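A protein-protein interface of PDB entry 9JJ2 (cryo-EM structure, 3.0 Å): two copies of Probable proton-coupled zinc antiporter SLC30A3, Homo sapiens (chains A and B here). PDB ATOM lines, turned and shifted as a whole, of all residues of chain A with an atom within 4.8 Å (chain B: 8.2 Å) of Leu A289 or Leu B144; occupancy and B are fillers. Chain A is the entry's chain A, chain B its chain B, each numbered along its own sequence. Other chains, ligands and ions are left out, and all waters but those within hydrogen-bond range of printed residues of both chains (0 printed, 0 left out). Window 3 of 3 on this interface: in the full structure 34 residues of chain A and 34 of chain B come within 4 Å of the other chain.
O of Leu A292 is in hydrogen-bond range of NH1 of Arg B140 (2.9 Å).
The backbone carbonyl oxygen (O) of Trp B138 is in hydrogen-bond range of the side-chain hydroxyl (OG) of Ser B141 (2.8 Å). The guanidinium group (NH2) of Arg B140 is in hydrogen-bond range of the backbone carbonyl oxygen (O) of Ile B291, 3.5 Å away. The backbone carbonyl oxygen (O) of Leu B326 lies within hydrogen-bond range of the guanidinium group (NE) of Arg B140 (3.0 Å). OG of Ser B141 sits at hydrogen-bond distance from OE1 of Glu B142 (3.3 Å).
Leu A289 touches Leu B144. Met A293 touches Met B134. Met A293 touches Trp B138. Met A293 touches Arg B140 (SD to CB, 3.8 Å). Met A293 touches Ser B141 (SD to N, 3.9 Å). CG of Met A293 touches CD1 of Leu B144, at 3.5 Å.
Leu A289 touches just one residue of chain B: Leu B144 (3.8 Å). Ser B122 touches none of the printed residues of chain A. Of the printed residues of chain A, Met B134 touches Met A293. Of the printed residues of chain A, Trp B138 touches Met A293 (3.5 Å). Of the printed residues of chain A, Arg B140 touches Leu A292 and Met A293. Of chain A, only Leu A289 and Met A293 come within 4 Å of Leu B144. Val B151 touches none of the printed residues of chain A. The nearest residue of chain B that does not touch Leu A289 is Met B134 (5.6 Å). The nearest residue of chain A that does not touch Leu B144 is Leu A292 (4.3 Å).
Of the 22 printed residues of chain B, 5 touch a printed residue of chain A. Among the printed residues, 7 pairs touch across the chains. Among the printed residues, no Asp or Glu carboxylate lies within 4 Å of a Lys or Arg side-chain nitrogen of the other chain.
Positions printed for both chains: 288, 291 and 292. Of the 7 pairs that touch across the chains among the printed residues, none has its exchanged pair printed and touching as well.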
ATOM      1  N   LEU A 285     -19.221  10.957  16.046  1.00  0.00           N
ATOM      2  CA  LEU A 285     -18.080  10.055  15.972  1.00  0.00           C
ATOM      3  C   LEU A 285     -17.243  10.349  14.736  1.00  0.00           C
ATOM      4  O   LEU A 285     -16.010  10.342  14.799  1.00  0.00           O
ATOM      5  CB  LEU A 285     -18.569   8.603  15.990  1.00  0.00           C
ATOM      6  CG  LEU A 285     -17.647   7.373  16.002  1.00  0.00           C
ATOM      7  CD1 LEU A 285     -16.778   7.206  14.760  1.00  0.00           C
ATOM      8  CD2 LEU A 285     -16.778   7.405  17.249  1.00  0.00           C
ATOM      9  N   ARG A 286     -17.896  10.611  13.602  1.00  0.00           N
ATOM     10  CA  ARG A 286     -17.151  10.915  12.383  1.00  0.00           C
ATOM     11  C   ARG A 286     -16.341  12.199  12.531  1.00  0.00           C
ATOM     12  O   ARG A 286     -15.169  12.254  12.134  1.00  0.00           O
ATOM     13  CB  ARG A 286     -18.113  11.010  11.199  1.00  0.00           C
ATOM     14  CG  ARG A 286     -17.787  12.103  10.201  1.00  0.00           C
ATOM     15  CD  ARG A 286     -18.455  11.834   8.866  1.00  0.00           C
ATOM     16  NE  ARG A 286     -19.909  11.856   8.972  1.00  0.00           N
ATOM     17  CZ  ARG A 286     -20.652  12.952   8.887  1.00  0.00           C
ATOM     18  NH1 ARG A 286     -20.108  14.143   8.701  1.00  0.00           N
ATOM     19  NH2 ARG A 286     -21.973  12.849   8.991  1.00  0.00           N
ATOM     20  N   ASP A 287     -16.945  13.240  13.108  1.00  0.00           N
ATOM     21  CA  ASP A 287     -16.226  14.497  13.303  1.00  0.00           C
ATOM     22  C   ASP A 287     -15.047  14.317  14.250  1.00  0.00           C
ATOM     23  O   ASP A 287     -13.952  14.840  14.001  1.00  0.00           O
ATOM     24  CB  ASP A 287     -17.174  15.569  13.833  1.00  0.00           C
ATOM     25  CG  ASP A 287     -18.014  16.190  12.742  1.00  0.00           C
ATOM     26  OD1 ASP A 287     -17.831  15.813  11.566  1.00  0.00           O
ATOM     27  OD2 ASP A 287     -18.860  17.054  13.056  1.00  0.00           O
ATOM     28  N   VAL A 288     -15.253  13.582  15.342  1.00  0.00           N
ATOM     29  CA  VAL A 288     -14.174  13.338  16.294  1.00  0.00           C
ATOM     30  C   VAL A 288     -13.047  12.563  15.628  1.00  0.00           C
ATOM     31  O   VAL A 288     -11.864  12.856  15.836  1.00  0.00           O
ATOM     32  CB  VAL A 288     -14.721  12.602  17.531  1.00  0.00           C
ATOM     33  CG1 VAL A 288     -13.621  11.825  18.226  1.00  0.00           C
ATOM     34  CG2 VAL A 288     -15.367  13.587  18.485  1.00  0.00           C
ATOM     35  N   LEU A 289     -13.396  11.563  14.818  1.00  0.00           N
ATOM     36  CA  LEU A 289     -12.381  10.776  14.131  1.00  0.00           C
ATOM     37  C   LEU A 289     -11.573  11.637  13.174  1.00  0.00           C
ATOM     38  O   LEU A 289     -10.346  11.517  13.108  1.00  0.00           O
ATOM     39  CB  LEU A 289     -13.037   9.616  13.386  1.00  0.00           C
ATOM     40  CG  LEU A 289     -13.201   8.312  14.167  1.00  0.00           C
ATOM     41  CD1 LEU A 289     -13.267   7.129  13.219  1.00  0.00           C
ATOM     42  CD2 LEU A 289     -12.079   8.132  15.176  1.00  0.00           C
ATOM     43  N   ARG A 290     -12.242  12.518  12.425  1.00  0.00           N
ATOM     44  CA  ARG A 290     -11.514  13.405  11.524  1.00  0.00           C
ATOM     45  C   ARG A 290     -10.581  14.333  12.293  1.00  0.00           C
ATOM     46  O   ARG A 290      -9.418  14.518  11.910  1.00  0.00           O
ATOM     47  CB  ARG A 290     -12.492  14.216  10.676  1.00  0.00           C
ATOM     48  CG  ARG A 290     -12.056  15.652  10.436  1.00  0.00           C
ATOM     49  CD  ARG A 290     -12.360  16.104   9.025  1.00  0.00           C
ATOM     50  NE  ARG A 290     -11.749  15.234   8.029  1.00  0.00           N
ATOM     51  CZ  ARG A 290     -11.898  15.380   6.721  1.00  0.00           C
ATOM     52  NH1 ARG A 290     -12.640  16.352   6.216  1.00  0.00           N
ATOM     53  NH2 ARG A 290     -11.289  14.531   5.899  1.00  0.00           N
ATOM     54  N   ILE A 291     -11.066  14.908  13.395  1.00  0.00           N
ATOM     55  CA  ILE A 291     -10.241  15.833  14.166  1.00  0.00           C
ATOM     56  C   ILE A 291      -9.021  15.116  14.726  1.00  0.00           C
ATOM     57  O   ILE A 291      -7.899  15.632  14.671  1.00  0.00           O
ATOM     58  CB  ILE A 291     -11.077  16.490  15.280  1.00  0.00           C
ATOM     59  CG1 ILE A 291     -11.777  17.737  14.748  1.00  0.00           C
ATOM     60  CG2 ILE A 291     -10.201  16.860  16.459  1.00  0.00           C
ATOM     61  CD1 ILE A 291     -12.495  18.520  15.812  1.00  0.00           C
ATOM     62  N   LEU A 292      -9.216  13.909  15.259  1.00  0.00           N
ATOM     63  CA  LEU A 292      -8.098  13.163  15.826  1.00  0.00           C
ATOM     64  C   LEU A 292      -7.127  12.691  14.752  1.00  0.00           C
ATOM     65  O   LEU A 292      -5.921  12.617  15.004  1.00  0.00           O
ATOM     66  CB  LEU A 292      -8.615  11.977  16.634  1.00  0.00           C
ATOM     67  CG  LEU A 292      -9.347  12.326  17.929  1.00  0.00           C
ATOM     68  CD1 LEU A 292      -9.552  11.084  18.771  1.00  0.00           C
ATOM     69  CD2 LEU A 292      -8.585  13.378  18.706  1.00  0.00           C
ATOM     70  N   MET A 293      -7.621  12.368  13.558  1.00  0.00           N
ATOM     71  CA  MET A 293      -6.741  11.989  12.462  1.00  0.00           C
ATOM     72  C   MET A 293      -6.092  13.190  11.798  1.00  0.00           C
ATOM     73  O   MET A 293      -5.262  13.005  10.902  1.00  0.00           O
ATOM     74  CB  MET A 293      -7.506  11.179  11.416  1.00  0.00           C
ATOM     75  CG  MET A 293      -7.779   9.750  11.830  1.00  0.00           C
ATOM     76  SD  MET A 293      -6.462   8.624  11.343  1.00  0.00           S
ATOM     77  CE  MET A 293      -6.488   8.830   9.571  1.00  0.00           C
ATOM     78  N   GLY B 118      -3.401  -3.455  14.190  1.00  0.00           N
ATOM     79  CA  GLY B 118      -3.306  -2.019  14.011  1.00  0.00           C
ATOM     80  C   GLY B 118      -2.004  -1.610  13.352  1.00  0.00           C
ATOM     81  O   GLY B 118      -1.988  -0.742  12.479  1.00  0.00           O
ATOM     82  N   SER B 122      -1.818   0.152   9.752  1.00  0.00           N
ATOM     83  CA  SER B 122      -1.113   1.423   9.654  1.00  0.00           C
ATOM     84  C   SER B 122      -0.005   1.366   8.613  1.00  0.00           C
ATOM     85  O   SER B 122       0.205   2.328   7.867  1.00  0.00           O
ATOM     86  CB  SER B 122      -0.551   1.800  11.022  1.00  0.00           C
ATOM     87  OG  SER B 122       0.818   1.451  11.125  1.00  0.00           O
ATOM     88  N   MET B 134      -6.586  15.345   4.037  1.00  0.00           N
ATOM     89  CA  MET B 134      -5.673  14.859   5.072  1.00  0.00           C
ATOM     90  C   MET B 134      -4.293  15.391   4.705  1.00  0.00           C
ATOM     91  O   MET B 134      -3.520  14.715   4.022  1.00  0.00           O
ATOM     92  CB  MET B 134      -5.690  13.339   5.169  1.00  0.00           C
ATOM     93  CG  MET B 134      -6.989  12.762   5.690  1.00  0.00           C
ATOM     94  SD  MET B 134      -6.877  12.296   7.423  1.00  0.00           S
ATOM     95  CE  MET B 134      -8.604  12.053   7.818  1.00  0.00           C
ATOM     96  N   TRP B 138      -1.758   9.731   6.838  1.00  0.00           N
ATOM     97  CA  TRP B 138      -2.556   8.823   7.649  1.00  0.00           C
ATOM     98  C   TRP B 138      -1.734   8.238   8.789  1.00  0.00           C
ATOM     99  O   TRP B 138      -1.910   7.075   9.155  1.00  0.00           O
ATOM    100  CB  TRP B 138      -3.147   7.705   6.793  1.00  0.00           C
ATOM    101  CG  TRP B 138      -3.865   8.194   5.583  1.00  0.00           C
ATOM    102  CD1 TRP B 138      -3.309   8.648   4.426  1.00  0.00           C
ATOM    103  CD2 TRP B 138      -5.280   8.270   5.406  1.00  0.00           C
ATOM    104  NE1 TRP B 138      -4.292   9.009   3.539  1.00  0.00           N
ATOM    105  CE2 TRP B 138      -5.512   8.786   4.118  1.00  0.00           C
ATOM    106  CE3 TRP B 138      -6.375   7.954   6.212  1.00  0.00           C
ATOM    107  CZ2 TRP B 138      -6.792   8.991   3.619  1.00  0.00           C
ATOM    108  CZ3 TRP B 138      -7.643   8.159   5.717  1.00  0.00           C
ATOM    109  CH2 TRP B 138      -7.843   8.673   4.432  1.00  0.00           C
ATOM    110  N   HIS B 139      -0.839   9.035   9.367  1.00  0.00           N
ATOM    111  CA  HIS B 139       0.049   8.536  10.405  1.00  0.00           C
ATOM    112  C   HIS B 139      -0.604   8.479  11.778  1.00  0.00           C
ATOM    113  O   HIS B 139       0.010   7.960  12.713  1.00  0.00           O
ATOM    114  CB  HIS B 139       1.307   9.399  10.467  1.00  0.00           C
ATOM    115  CG  HIS B 139       2.023   9.505   9.158  1.00  0.00           C
ATOM    116  ND1 HIS B 139       2.621   8.425   8.548  1.00  0.00           N
ATOM    117  CD2 HIS B 139       2.232  10.563   8.340  1.00  0.00           C
ATOM    118  CE1 HIS B 139       3.171   8.813   7.411  1.00  0.00           C
ATOM    119  NE2 HIS B 139       2.950  10.106   7.262  1.00  0.00           N
ATOM    120  N   ARG B 140      -1.819   8.999  11.927  1.00  0.00           N
ATOM    121  CA  ARG B 140      -2.540   8.876  13.186  1.00  0.00           C
ATOM    122  C   ARG B 140      -3.275   7.550  13.304  1.00  0.00           C
ATOM    123  O   ARG B 140      -3.890   7.286  14.346  1.00  0.00           O
ATOM    124  CB  ARG B 140      -3.526  10.033  13.341  1.00  0.00           C
ATOM    125  CG  ARG B 140      -2.887  11.319  13.826  1.00  0.00           C
ATOM    126  CD  ARG B 140      -2.869  11.382  15.339  1.00  0.00           C
ATOM    127  NE  ARG B 140      -1.969  12.414  15.831  1.00  0.00           N
ATOM    128  CZ  ARG B 140      -2.361  13.596  16.282  1.00  0.00           C
ATOM    129  NH1 ARG B 140      -3.638  13.934  16.317  1.00  0.00           N
ATOM    130  NH2 ARG B 140      -1.448  14.462  16.714  1.00  0.00           N
ATOM    131  N   SER B 141      -3.229   6.720  12.260  1.00  0.00           N
ATOM    132  CA  SER B 141      -3.852   5.405  12.329  1.00  0.00           C
ATOM    133  C   SER B 141      -3.189   4.532  13.383  1.00  0.00           C
ATOM    134  O   SER B 141      -3.866   3.724  14.022  1.00  0.00           O
ATOM    135  CB  SER B 141      -3.796   4.724  10.963  1.00  0.00           C
ATOM    136  OG  SER B 141      -2.470   4.680  10.472  1.00  0.00           O
ATOM    137  N   GLU B 142      -1.876   4.678  13.580  1.00  0.00           N
ATOM    138  CA  GLU B 142      -1.200   3.938  14.642  1.00  0.00           C
ATOM    139  C   GLU B 142      -1.834   4.235  15.994  1.00  0.00           C
ATOM    140  O   GLU B 142      -2.212   3.320  16.736  1.00  0.00           O
ATOM    141  CB  GLU B 142       0.289   4.291  14.688  1.00  0.00           C
ATOM    142  CG  GLU B 142       1.191   3.665  13.627  1.00  0.00           C
ATOM    143  CD  GLU B 142       1.120   4.352  12.276  1.00  0.00           C
ATOM    144  OE1 GLU B 142       0.295   5.266  12.096  1.00  0.00           O
ATOM    145  OE2 GLU B 142       1.916   3.984  11.388  1.00  0.00           O
ATOM    146  N   THR B 143      -1.957   5.521  16.326  1.00  0.00           N
ATOM    147  CA  THR B 143      -2.511   5.910  17.616  1.00  0.00           C
ATOM    148  C   THR B 143      -3.973   5.506  17.734  1.00  0.00           C
ATOM    149  O   THR B 143      -4.410   5.050  18.796  1.00  0.00           O
ATOM    150  CB  THR B 143      -2.351   7.414  17.818  1.00  0.00           C
ATOM    151  OG1 THR B 143      -1.016   7.801  17.478  1.00  0.00           O
ATOM    152  CG2 THR B 143      -2.623   7.782  19.261  1.00  0.00           C
ATOM    153  N   LEU B 144      -4.745   5.667  16.658  1.00  0.00           N
ATOM    154  CA  LEU B 144      -6.153   5.290  16.718  1.00  0.00           C
ATOM    155  C   LEU B 144      -6.314   3.790  16.928  1.00  0.00           C
ATOM    156  O   LEU B 144      -7.166   3.354  17.710  1.00  0.00           O
ATOM    157  CB  LEU B 144      -6.871   5.745  15.451  1.00  0.00           C
ATOM    158  CG  LEU B 144      -7.191   7.241  15.374  1.00  0.00           C
ATOM    159  CD1 LEU B 144      -8.387   7.474  14.475  1.00  0.00           C
ATOM    160  CD2 LEU B 144      -7.440   7.827  16.752  1.00  0.00           C
ATOM    161  N   GLY B 145      -5.497   2.982  16.251  1.00  0.00           N
ATOM    162  CA  GLY B 145      -5.562   1.545  16.449  1.00  0.00           C
ATOM    163  C   GLY B 145      -5.134   1.128  17.841  1.00  0.00           C
ATOM    164  O   GLY B 145      -5.729   0.227  18.438  1.00  0.00           O
ATOM    165  N   ALA B 146      -4.096   1.773  18.379  1.00  0.00           N
ATOM    166  CA  ALA B 146      -3.684   1.475  19.747  1.00  0.00           C
ATOM    167  C   ALA B 146      -4.788   1.818  20.738  1.00  0.00           C
ATOM    168  O   ALA B 146      -5.066   1.047  21.667  1.00  0.00           O
ATOM    169  CB  ALA B 146      -2.402   2.232  20.086  1.00  0.00           C
ATOM    170  N   LEU B 147      -5.438   2.967  20.548  1.00  0.00           N
ATOM    171  CA  LEU B 147      -6.539   3.350  21.424  1.00  0.00           C
ATOM    172  C   LEU B 147      -7.699   2.369  21.313  1.00  0.00           C
ATOM    173  O   LEU B 147      -8.317   2.012  22.321  1.00  0.00           O
ATOM    174  CB  LEU B 147      -6.998   4.768  21.093  1.00  0.00           C
ATOM    175  CG  LEU B 147      -8.034   5.370  22.038  1.00  0.00           C
ATOM    176  CD1 LEU B 147      -7.451   5.520  23.428  1.00  0.00           C
ATOM    177  CD2 LEU B 147      -8.514   6.707  21.510  1.00  0.00           C
ATOM    178  N   ALA B 148      -8.013   1.929  20.093  1.00  0.00           N
ATOM    179  CA  ALA B 148      -9.084   0.954  19.913  1.00  0.00           C
ATOM    180  C   ALA B 148      -8.750  -0.366  20.596  1.00  0.00           C
ATOM    181  O   ALA B 148      -9.618  -0.990  21.218  1.00  0.00           O
ATOM    182  CB  ALA B 148      -9.350   0.736  18.425  1.00  0.00           C
ATOM    183  N   SER B 149      -7.497  -0.809  20.483  1.00  0.00           N
ATOM    184  CA  SER B 149      -7.092  -2.046  21.143  1.00  0.00           C
ATOM    185  C   SER B 149      -7.205  -1.921  22.656  1.00  0.00           C
ATOM    186  O   SER B 149      -7.668  -2.848  23.330  1.00  0.00           O
ATOM    187  CB  SER B 149      -5.668  -2.416  20.733  1.00  0.00           C
ATOM    188  OG  SER B 149      -4.719  -1.905  21.648  1.00  0.00           O
ATOM    189  N   VAL B 150      -6.798  -0.777  23.209  1.00  0.00           N
ATOM    190  CA  VAL B 150      -6.926  -0.570  24.650  1.00  0.00           C
ATOM    191  C   VAL B 150      -8.394  -0.567  25.062  1.00  0.00           C
ATOM    192  O   VAL B 150      -8.770  -1.154  26.085  1.00  0.00           O
ATOM    193  CB  VAL B 150      -6.215   0.729  25.067  1.00  0.00           C
ATOM    194  CG1 VAL B 150      -6.571   1.092  26.494  1.00  0.00           C
ATOM    195  CG2 VAL B 150      -4.713   0.573  24.919  1.00  0.00           C
ATOM    196  N   VAL B 151      -9.245   0.088  24.273  1.00  0.00           N
ATOM    197  CA  VAL B 151     -10.667   0.147  24.596  1.00  0.00           C
ATOM    198  C   VAL B 151     -11.275  -1.251  24.587  1.00  0.00           C
ATOM    199  O   VAL B 151     -12.069  -1.602  25.467  1.00  0.00           O
ATOM    200  CB  VAL B 151     -11.394   1.094  23.623  1.00  0.00           C
ATOM    201  CG1 VAL B 151     -12.848   0.683  23.451  1.00  0.00           C
ATOM    202  CG2 VAL B 151     -11.296   2.526  24.115  1.00  0.00           C
ATOM    203  N   VAL B 288      -0.652   7.240  24.204  1.00  0.00           N
ATOM    204  CA  VAL B 288      -1.678   7.532  23.208  1.00  0.00           C
ATOM    205  C   VAL B 288      -2.422   8.806  23.574  1.00  0.00           C
ATOM    206  O   VAL B 288      -2.701   9.650  22.714  1.00  0.00           O
ATOM    207  CB  VAL B 288      -2.634   6.332  23.070  1.00  0.00           C
ATOM    208  CG1 VAL B 288      -3.999   6.784  22.588  1.00  0.00           C
ATOM    209  CG2 VAL B 288      -2.046   5.301  22.130  1.00  0.00           C
ATOM    210  N   ILE B 291      -0.217  11.843  22.828  1.00  0.00           N
ATOM    211  CA  ILE B 291      -0.120  12.092  21.391  1.00  0.00           C
ATOM    212  C   ILE B 291      -1.409  12.710  20.869  1.00  0.00           C
ATOM    213  O   ILE B 291      -1.382  13.664  20.084  1.00  0.00           O
ATOM    214  CB  ILE B 291       0.231  10.790  20.647  1.00  0.00           C
ATOM    215  CG1 ILE B 291       1.744  10.624  20.556  1.00  0.00           C
ATOM    216  CG2 ILE B 291      -0.366  10.785  19.258  1.00  0.00           C
ATOM    217  CD1 ILE B 291       2.172   9.235  20.168  1.00  0.00           C
ATOM    218  N   LEU B 292      -2.557  12.185  21.304  1.00  0.00           N
ATOM    219  CA  LEU B 292      -3.833  12.710  20.832  1.00  0.00           C
ATOM    220  C   LEU B 292      -4.098  14.116  21.353  1.00  0.00           C
ATOM    221  O   LEU B 292      -4.696  14.930  20.643  1.00  0.00           O
ATOM    222  CB  LEU B 292      -4.970  11.773  21.231  1.00  0.00           C
ATOM    223  CG  LEU B 292      -5.033  10.446  20.476  1.00  0.00           C
ATOM    224  CD1 LEU B 292      -6.335   9.734  20.774  1.00  0.00           C
ATOM    225  CD2 LEU B 292      -4.883  10.675  18.987  1.00  0.00           C
ATOM    226  N   LEU B 326       2.729  13.284  15.356  1.00  0.00           N
ATOM    227  CA  LEU B 326       1.634  12.556  14.727  1.00  0.00           C
ATOM    228  C   LEU B 326       1.517  11.151  15.298  1.00  0.00           C
ATOM    229  O   LEU B 326       0.409  10.668  15.556  1.00  0.00           O
ATOM    230  CB  LEU B 326       1.838  12.499  13.218  1.00  0.00           C
ATOM    231  CG  LEU B 326       1.390  13.711  12.408  1.00  0.00           C
ATOM    232  CD1 LEU B 326       1.130  13.300  10.979  1.00  0.00           C
ATOM    233  CD2 LEU B 326       0.155  14.330  13.017  1.00  0.00           C
ATOM    234  N   THR B 327       2.646  10.485  15.499  1.00  0.00           N
ATOM    235  CA  THR B 327       2.677   9.144  16.064  1.00  0.00           C
ATOM    236  C   THR B 327       3.975   9.021  16.857  1.00  0.00           C
ATOM    237  O   THR B 327       4.628  10.027  17.154  1.00  0.00           O
ATOM    238  CB  THR B 327       2.521   8.094  14.948  1.00  0.00           C
ATOM    239  OG1 THR B 327       2.494   6.778  15.512  1.00  0.00           O
ATOM    240  CG2 THR B 327       3.670   8.190  13.965  1.00  0.00           C
